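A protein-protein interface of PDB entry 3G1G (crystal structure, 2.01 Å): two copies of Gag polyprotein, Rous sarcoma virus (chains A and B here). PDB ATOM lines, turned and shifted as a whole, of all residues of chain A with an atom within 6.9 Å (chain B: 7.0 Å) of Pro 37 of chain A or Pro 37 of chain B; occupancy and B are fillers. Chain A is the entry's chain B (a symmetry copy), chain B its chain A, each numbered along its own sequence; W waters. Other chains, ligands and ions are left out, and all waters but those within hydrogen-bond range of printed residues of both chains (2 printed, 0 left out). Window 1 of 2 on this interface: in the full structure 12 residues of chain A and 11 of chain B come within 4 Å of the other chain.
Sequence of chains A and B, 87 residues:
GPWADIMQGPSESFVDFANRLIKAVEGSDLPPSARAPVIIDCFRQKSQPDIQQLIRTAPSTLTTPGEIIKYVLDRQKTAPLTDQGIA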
ATOM      1  N   PRO A  32      27.766 -17.641  11.890  1.00  0.00           N
ATOM      2  CA  PRO A  32      27.991 -17.526  13.330  1.00  0.00           C
ATOM      3  C   PRO A  32      26.860 -18.076  14.152  1.00  0.00           C
ATOM      4  O   PRO A  32      27.081 -18.612  15.270  1.00  0.00           O
ATOM      5  CB  PRO A  32      28.071 -15.996  13.569  1.00  0.00           C
ATOM      6  CG  PRO A  32      28.007 -15.349  12.186  1.00  0.00           C
ATOM      7  CD  PRO A  32      28.238 -16.438  11.176  1.00  0.00           C
ATOM      8  N   SER A  33      25.641 -17.931  13.641  1.00  0.00           N
ATOM      9  CA  SER A  33      24.494 -18.394  14.440  1.00  0.00           C
ATOM     10  C   SER A  33      24.422 -19.943  14.492  1.00  0.00           C
ATOM     11  O   SER A  33      23.734 -20.491  15.345  1.00  0.00           O
ATOM     12  CB  SER A  33      23.178 -17.816  13.908  1.00  0.00           C
ATOM     13  OG  SER A  33      22.778 -18.574  12.774  1.00  0.00           O
ATOM     14  N   ALA A  34      25.132 -20.617  13.579  1.00  0.00           N
ATOM     15  CA  ALA A  34      25.193 -22.075  13.562  1.00  0.00           C
ATOM     16  C   ALA A  34      26.308 -22.686  14.438  1.00  0.00           C
ATOM     17  O   ALA A  34      26.333 -23.898  14.628  1.00  0.00           O
ATOM     18  CB  ALA A  34      25.347 -22.575  12.126  1.00  0.00           C
ATOM     19  N   ARG A  35      27.228 -21.859  14.942  1.00  0.00           N
ATOM     20  CA  ARG A  35      28.430 -22.356  15.678  1.00  0.00           C
ATOM     21  C   ARG A  35      28.067 -23.048  16.969  1.00  0.00           C
ATOM     22  O   ARG A  35      28.476 -24.194  17.175  1.00  0.00           O
ATOM     23  CB  ARG A  35      29.425 -21.222  15.970  1.00  0.00           C
ATOM     24  CG  ARG A  35      29.985 -20.605  14.665  1.00  0.00           C
ATOM     25  CD  ARG A  35      30.918 -19.446  14.996  1.00  0.00           C
ATOM     26  NE  ARG A  35      31.446 -18.800  13.789  1.00  0.00           N
ATOM     27  CZ  ARG A  35      31.884 -17.533  13.747  1.00  0.00           C
ATOM     28  NH1 ARG A  35      31.828 -16.749  14.829  1.00  0.00           N
ATOM     29  NH2 ARG A  35      32.346 -17.034  12.612  1.00  0.00           N
ATOM     30  N   ALA A  36      27.291 -22.380  17.834  1.00  0.00           N
ATOM     31  CA  ALA A  36      27.060 -22.936  19.139  1.00  0.00           C
ATOM     32  C   ALA A  36      26.240 -24.232  19.042  1.00  0.00           C
ATOM     33  O   ALA A  36      26.568 -25.204  19.736  1.00  0.00           O
ATOM     34  CB  ALA A  36      26.433 -21.893  20.146  1.00  0.00           C
ATOM     35  N   PRO A  37      25.185 -24.253  18.191  1.00  0.00           N
ATOM     36  CA  PRO A  37      24.475 -25.553  18.084  1.00  0.00           C
ATOM     37  C   PRO A  37      25.344 -26.681  17.520  1.00  0.00           C
ATOM     38  O   PRO A  37      25.214 -27.820  17.984  1.00  0.00           O
ATOM     39  CB  PRO A  37      23.298 -25.283  17.134  1.00  0.00           C
ATOM     40  CG  PRO A  37      23.242 -23.832  16.886  1.00  0.00           C
ATOM     41  CD  PRO A  37      24.453 -23.143  17.520  1.00  0.00           C
ATOM     42  N   VAL A  38      26.159 -26.387  16.502  1.00  0.00           N
ATOM     43  CA  VAL A  38      27.103 -27.377  15.949  1.00  0.00           C
ATOM     44  C   VAL A  38      28.087 -27.840  17.018  1.00  0.00           C
ATOM     45  O   VAL A  38      28.319 -29.042  17.203  1.00  0.00           O
ATOM     46  CB  VAL A  38      27.786 -26.897  14.661  1.00  0.00           C
ATOM     47  CG1 VAL A  38      29.020 -27.765  14.325  1.00  0.00           C
ATOM     48  CG2 VAL A  38      26.760 -26.999  13.533  1.00  0.00           C
ATOM     49  N   ILE A  39      28.643 -26.879  17.759  1.00  0.00           N
ATOM     50  CA  ILE A  39      29.520 -27.230  18.872  1.00  0.00           C
ATOM     51  C   ILE A  39      28.869 -28.154  19.894  1.00  0.00           C
ATOM     52  O   ILE A  39      29.442 -29.174  20.282  1.00  0.00           O
ATOM     53  CB  ILE A  39      30.140 -25.991  19.545  1.00  0.00           C
ATOM     54  CG1 ILE A  39      31.150 -25.378  18.600  1.00  0.00           C
ATOM     55  CG2 ILE A  39      30.907 -26.363  20.775  1.00  0.00           C
ATOM     56  CD1 ILE A  39      31.377 -23.845  18.903  1.00  0.00           C
ATOM     57  N   ILE A  40      27.682 -27.810  20.349  1.00  0.00           N
ATOM     58  CA  ILE A  40      27.053 -28.644  21.386  1.00  0.00           C
ATOM     59  C   ILE A  40      26.764 -30.037  20.788  1.00  0.00           C
ATOM     60  O   ILE A  40      27.030 -31.054  21.425  1.00  0.00           O
ATOM     61  CB  ILE A  40      25.829 -27.954  21.946  1.00  0.00           C
ATOM     62  CG1 ILE A  40      26.295 -26.687  22.696  1.00  0.00           C
ATOM     63  CG2 ILE A  40      25.000 -28.929  22.856  1.00  0.00           C
ATOM     64  CD1 ILE A  40      25.150 -25.653  23.009  1.00  0.00           C
ATOM     65  N   ASP A  41      26.305 -30.081  19.542  1.00  0.00           N
ATOM     66  CA  ASP A  41      26.022 -31.363  18.875  1.00  0.00           C
ATOM     67  C   ASP A  41      27.286 -32.257  18.848  1.00  0.00           C
ATOM     68  O   ASP A  41      27.224 -33.475  19.041  1.00  0.00           O
ATOM     69  CB  ASP A  41      25.504 -31.145  17.452  1.00  0.00           C
ATOM     70  CG  ASP A  41      25.245 -32.454  16.734  1.00  0.00           C
ATOM     71  OD1 ASP A  41      24.320 -33.168  17.147  1.00  0.00           O
ATOM     72  OD2 ASP A  41      25.964 -32.778  15.764  1.00  0.00           O
ATOM     73  N   CYS A  42      28.428 -31.640  18.567  1.00  0.00           N
ATOM     74  CA  CYS A  42      29.681 -32.376  18.528  1.00  0.00           C
ATOM     75  C   CYS A  42      30.122 -32.838  19.903  1.00  0.00           C
ATOM     76  O   CYS A  42      30.668 -33.935  20.039  1.00  0.00           O
ATOM     77  CB  CYS A  42      30.749 -31.532  17.870  1.00  0.00           C
ATOM     78  SG  CYS A  42      30.498 -31.508  16.122  1.00  0.00           S
ATOM     79  N   GLN A  45      28.121 -36.043  20.375  1.00  0.00           N
ATOM     80  CA  GLN A  45      28.375 -37.244  19.572  1.00  0.00           C
ATOM     81  C   GLN A  45      29.864 -37.588  19.456  1.00  0.00           C
ATOM     82  O   GLN A  45      30.204 -38.688  19.074  1.00  0.00           O
ATOM     83  CB  GLN A  45      27.762 -37.135  18.159  1.00  0.00           C
ATOM     84  CG  GLN A  45      26.346 -36.538  18.078  1.00  0.00           C
ATOM     85  CD  GLN A  45      25.851 -36.405  16.634  1.00  0.00           C
ATOM     86  OE1 GLN A  45      26.506 -36.861  15.699  1.00  0.00           O
ATOM     87  NE2 GLN A  45      24.689 -35.783  16.455  1.00  0.00           N
ATOM     88  N   THR A  63      22.342 -24.285  26.928  1.00  0.00           N
ATOM     89  CA  THR A  63      22.378 -24.156  25.471  1.00  0.00           C
ATOM     90  C   THR A  63      23.560 -23.359  24.960  1.00  0.00           C
ATOM     91  O   THR A  63      23.594 -22.981  23.791  1.00  0.00           O
ATOM     92  CB  THR A  63      21.083 -23.512  24.891  1.00  0.00           C
ATOM     93  OG1 THR A  63      20.927 -22.190  25.425  1.00  0.00           O
ATOM     94  CG2 THR A  63      19.829 -24.370  25.159  1.00  0.00           C
ATOM     95  N   PRO A  65      27.925 -23.502  24.713  1.00  0.00           N
ATOM     96  CA  PRO A  65      29.071 -24.385  24.933  1.00  0.00           C
ATOM     97  C   PRO A  65      29.706 -24.202  26.318  1.00  0.00           C
ATOM     98  O   PRO A  65      30.063 -25.194  26.949  1.00  0.00           O
ATOM     99  CB  PRO A  65      30.017 -24.011  23.783  1.00  0.00           C
ATOM    100  CG  PRO A  65      29.088 -23.576  22.700  1.00  0.00           C
ATOM    101  CD  PRO A  65      28.026 -22.790  23.420  1.00  0.00           C
ATOM    102  N   PRO B  32      25.151 -30.905   5.798  1.00  0.00           N
ATOM    103  CA  PRO B  32      23.983 -31.694   6.214  1.00  0.00           C
ATOM    104  C   PRO B  32      23.997 -31.989   7.715  1.00  0.00           C
ATOM    105  O   PRO B  32      22.934 -32.069   8.345  1.00  0.00           O
ATOM    106  CB  PRO B  32      24.138 -33.003   5.409  1.00  0.00           C
ATOM    107  CG  PRO B  32      24.817 -32.551   4.138  1.00  0.00           C
ATOM    108  CD  PRO B  32      25.825 -31.525   4.634  1.00  0.00           C
ATOM    109  N   SER B  33      25.202 -32.181   8.265  1.00  0.00           N
ATOM    110  CA  SER B  33      25.355 -32.593   9.681  1.00  0.00           C
ATOM    111  C   SER B  33      25.032 -31.438  10.631  1.00  0.00           C
ATOM    112  O   SER B  33      24.741 -31.660  11.815  1.00  0.00           O
ATOM    113  CB  SER B  33      26.777 -33.123   9.925  1.00  0.00           C
ATOM    114  OG  SER B  33      27.698 -32.072  10.113  1.00  0.00           O
ATOM    115  N   ALA B  34      25.069 -30.211  10.115  1.00  0.00           N
ATOM    116  CA  ALA B  34      24.667 -29.011  10.888  1.00  0.00           C
ATOM    117  C   ALA B  34      23.157 -28.702  10.868  1.00  0.00           C
ATOM    118  O   ALA B  34      22.709 -27.770  11.584  1.00  0.00           O
ATOM    119  CB  ALA B  34      25.431 -27.775  10.401  1.00  0.00           C
ATOM    120  N   ARG B  35      22.390 -29.425  10.041  1.00  0.00           N
ATOM    121  CA  ARG B  35      20.971 -29.075   9.825  1.00  0.00           C
ATOM    122  C   ARG B  35      20.160 -29.356  11.082  1.00  0.00           C
ATOM    123  O   ARG B  35      19.485 -28.481  11.598  1.00  0.00           O
ATOM    124  CB  ARG B  35      20.352 -29.865   8.635  1.00  0.00           C
ATOM    125  CG  ARG B  35      20.879 -29.523   7.310  1.00  0.00           C
ATOM    126  CD  ARG B  35      20.355 -30.572   6.313  1.00  0.00           C
ATOM    127  NE  ARG B  35      20.882 -30.301   4.997  1.00  0.00           N
ATOM    128  CZ  ARG B  35      20.885 -31.195   4.012  1.00  0.00           C
ATOM    129  NH1 ARG B  35      20.411 -32.418   4.222  1.00  0.00           N
ATOM    130  NH2 ARG B  35      21.401 -30.880   2.826  1.00  0.00           N
ATOM    131  N   ALA B  36      20.222 -30.580  11.579  1.00  0.00           N
ATOM    132  CA  ALA B  36      19.395 -30.920  12.742  1.00  0.00           C
ATOM    133  C   ALA B  36      19.679 -29.989  13.948  1.00  0.00           C
ATOM    134  O   ALA B  36      18.733 -29.433  14.539  1.00  0.00           O
ATOM    135  CB  ALA B  36      19.564 -32.416  13.096  1.00  0.00           C
ATOM    136  N   PRO B  37      20.968 -29.804  14.324  1.00  0.00           N
ATOM    137  CA  PRO B  37      21.284 -28.846  15.413  1.00  0.00           C
ATOM    138  C   PRO B  37      20.738 -27.451  15.197  1.00  0.00           C
ATOM    139  O   PRO B  37      20.182 -26.825  16.139  1.00  0.00           O
ATOM    140  CB  PRO B  37      22.831 -28.781  15.382  1.00  0.00           C
ATOM    141  CG  PRO B  37      23.268 -30.044  14.783  1.00  0.00           C
ATOM    142  CD  PRO B  37      22.123 -30.679  14.034  1.00  0.00           C
ATOM    143  N   VAL B  38      20.928 -26.939  13.989  1.00  0.00           N
ATOM    144  CA  VAL B  38      20.420 -25.617  13.637  1.00  0.00           C
ATOM    145  C   VAL B  38      18.900 -25.492  13.667  1.00  0.00           C
ATOM    146  O   VAL B  38      18.381 -24.488  14.160  1.00  0.00           O
ATOM    147  CB  VAL B  38      20.978 -25.097  12.277  1.00  0.00           C
ATOM    148  CG1 VAL B  38      20.313 -23.765  11.891  1.00  0.00           C
ATOM    149  CG2 VAL B  38      22.466 -24.894  12.424  1.00  0.00           C
ATOM    150  N   ILE B  39      18.193 -26.491  13.112  1.00  0.00           N
ATOM    151  CA  ILE B  39      16.746 -26.490  13.104  1.00  0.00           C
ATOM    152  C   ILE B  39      16.209 -26.474  14.543  1.00  0.00           C
ATOM    153  O   ILE B  39      15.315 -25.679  14.872  1.00  0.00           O
ATOM    154  CB  ILE B  39      16.181 -27.707  12.334  1.00  0.00           C
ATOM    155  CG1 ILE B  39      16.494 -27.573  10.841  1.00  0.00           C
ATOM    156  CG2 ILE B  39      14.663 -27.775  12.492  1.00  0.00           C
ATOM    157  CD1 ILE B  39      16.380 -28.926  10.101  1.00  0.00           C
ATOM    158  N   ILE B  40      16.745 -27.338  15.402  1.00  0.00           N
ATOM    159  CA  ILE B  40      16.281 -27.387  16.789  1.00  0.00           C
ATOM    160  C   ILE B  40      16.576 -26.064  17.509  1.00  0.00           C
ATOM    161  O   ILE B  40      15.744 -25.547  18.258  1.00  0.00           O
ATOM    162  CB  ILE B  40      16.803 -28.670  17.533  1.00  0.00           C
ATOM    163  CG1 ILE B  40      16.173 -29.915  16.907  1.00  0.00           C
ATOM    164  CG2 ILE B  40      16.435 -28.666  19.037  1.00  0.00           C
ATOM    165  CD1 ILE B  40      16.988 -31.173  17.246  1.00  0.00           C
ATOM    166  N   ASP B  41      17.726 -25.472  17.233  1.00  0.00           N
ATOM    167  CA  ASP B  41      18.056 -24.197  17.875  1.00  0.00           C
ATOM    168  C   ASP B  41      17.037 -23.105  17.463  1.00  0.00           C
ATOM    169  O   ASP B  41      16.611 -22.283  18.300  1.00  0.00           O
ATOM    170  CB  ASP B  41      19.499 -23.761  17.576  1.00  0.00           C
ATOM    171  CG  ASP B  41      19.839 -22.416  18.240  1.00  0.00           C
ATOM    172  OD1 ASP B  41      19.852 -22.362  19.485  1.00  0.00           O
ATOM    173  OD2 ASP B  41      20.036 -21.419  17.526  1.00  0.00           O
ATOM    174  N   CYS B  42      16.660 -23.119  16.170  1.00  0.00           N
ATOM    175  CA  CYS B  42      15.604 -22.263  15.650  1.00  0.00           C
ATOM    176  C   CYS B  42      14.223 -22.525  16.257  1.00  0.00           C
ATOM    177  O   CYS B  42      13.499 -21.559  16.517  1.00  0.00           O
ATOM    178  CB  CYS B  42      15.565 -22.306  14.122  1.00  0.00           C
ATOM    179  SG  CYS B  42      16.974 -21.400  13.415  1.00  0.00           S
ATOM    180  N   ARG B  44      13.854 -23.479  19.288  1.00  0.00           N
ATOM    181  CA  ARG B  44      13.984 -22.895  20.622  1.00  0.00           C
ATOM    182  C   ARG B  44      13.869 -21.378  20.618  1.00  0.00           C
ATOM    183  O   ARG B  44      13.281 -20.793  21.515  1.00  0.00           O
ATOM    184  CB  ARG B  44      15.307 -23.322  21.263  1.00  0.00           C
ATOM    185  CG  ARG B  44      15.179 -24.712  21.847  1.00  0.00           C
ATOM    186  CD  ARG B  44      16.345 -24.995  22.765  1.00  0.00           C
ATOM    187  NE  ARG B  44      17.581 -25.076  22.009  1.00  0.00           N
ATOM    188  CZ  ARG B  44      18.185 -26.221  21.710  1.00  0.00           C
ATOM    189  NH1 ARG B  44      17.650 -27.374  22.131  1.00  0.00           N
ATOM    190  NH2 ARG B  44      19.323 -26.214  21.007  1.00  0.00           N
ATOM    191  N   THR B  63      16.773 -35.429  19.722  1.00  0.00           N
ATOM    192  CA  THR B  63      17.756 -34.612  19.028  1.00  0.00           C
ATOM    193  C   THR B  63      17.518 -34.521  17.534  1.00  0.00           C
ATOM    194  O   THR B  63      18.342 -33.962  16.819  1.00  0.00           O
ATOM    195  CB  THR B  63      19.196 -35.113  19.293  1.00  0.00           C
ATOM    196  OG1 THR B  63      19.292 -36.505  18.946  1.00  0.00           O
ATOM    197  CG2 THR B  63      19.573 -34.930  20.748  1.00  0.00           C
ATOM    198  N   PRO B  65      14.708 -33.071  14.655  1.00  0.00           N
ATOM    199  CA  PRO B  65      13.572 -32.157  14.494  1.00  0.00           C
ATOM    200  C   PRO B  65      12.234 -32.916  14.596  1.00  0.00           C
ATOM    201  O   PRO B  65      11.295 -32.439  15.242  1.00  0.00           O
ATOM    202  CB  PRO B  65      13.785 -31.631  13.074  1.00  0.00           C
ATOM    203  CG  PRO B  65      15.260 -31.644  12.918  1.00  0.00           C
ATOM    204  CD  PRO B  65      15.666 -32.936  13.540  1.00  0.00           C
HETATM  205  O   HOH W   1      26.736 -30.865  14.003  1.00  0.00           O
HETATM  206  O   HOH W   2      21.119 -21.770  14.811  1.00  0.00           O
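The backbone carbonyl oxygen of Val 38 of chain B sits at hydrogen-bond distance from the side-chain sulfur of Cys 42 of chain B (3.5 Å).
The side-chain sulfur of Cys 42 of chain A sits at hydrogen-bond distance from the backbone carbonyl oxygen of Val 38 of chain A (3.5 Å).
The side-chain amide nitrogen (NE2) of Gln 45 of chain A sits at hydrogen-bond distance from the side-chain carboxylate (OD1) of Asp 41 of chain A, 2.7 Å away.
Among the printed residues, merely in contact across the chains: Ala 34 of chain A with Val 38 of chain B (3.7 Å), Pro 37 of chain A with Pro 37 of chain B (3.6 Å), Pro 37 of chain A with Asp 41 of chain B (3.8 Å), Val 38 of chain A with Ala 34 of chain B (3.5 Å), Asp 41 of chain A with Pro 37 of chain B (3.7 Å) and Thr 63 of chain A with Arg 44 of chain B (3.9 Å).
Pro 37 of chain B touches just these residues of chain A: Pro 37 and Asp 41.
Printed residues of chain A within 4 Å of Ala 34 of chain B: Val 38.
Of the printed residues of chain B, Val 38 of chain A touches Ala 34.
Of the printed residues of chain B, Asp 41 of chain A touches Pro 37.
Printed residues of chain B within 4 Å of Thr 63 of chain A: Arg 44 (3.9 Å).
Printed residues of chain B within 4 Å of Ala 34 of chain A: Val 38 (3.7 Å).
The nearest residue of chain B that does not touch Pro 37 of chain A is Val 38 of chain B (4.3 Å).
Of the 14 printed residues of chain A, 5 touch a printed residue of chain B.
Hydrophobic or aromatic side chains of chain A within 4 Å of the printed part of chain B: Ala 34, Pro 37 and Val 38.
Hydrophobic or aromatic side chains of chain B within 4 Å of the printed part of chain A: Ala 34, Pro 37 and Val 38.
Among the printed residues, no Asp or Glu carboxylate lies within 4 Å of a Lys or Arg side-chain nitrogen of the other chain.
Ala 34 of chain A touches Val 38 of chain B, and with the chains exchanged Val 38 of chain A touches Ala 34 of chain B.
Pro 37 of chain A touches its own counterpart, Pro 37 of chain B.
Pro 37 of chain A touches Asp 41 of chain B, and with the chains exchanged Asp 41 of chain A touches Pro 37 of chain B.
13 positions are printed for both chains.
Water W1 lies within hydrogen-bond range of the side-chain carboxylate (OD2) of Asp 41 of chain A (2.7 Å) and the backbone carbonyl oxygen (O) of Ser 33 of chain B (3.1 Å).
Water W2 bridges the side-chain carboxylate of Asp 41 of chain B (2.9 Å) and the backbone carbonyl oxygen of Ser 33 of chain A (3.0 Å).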
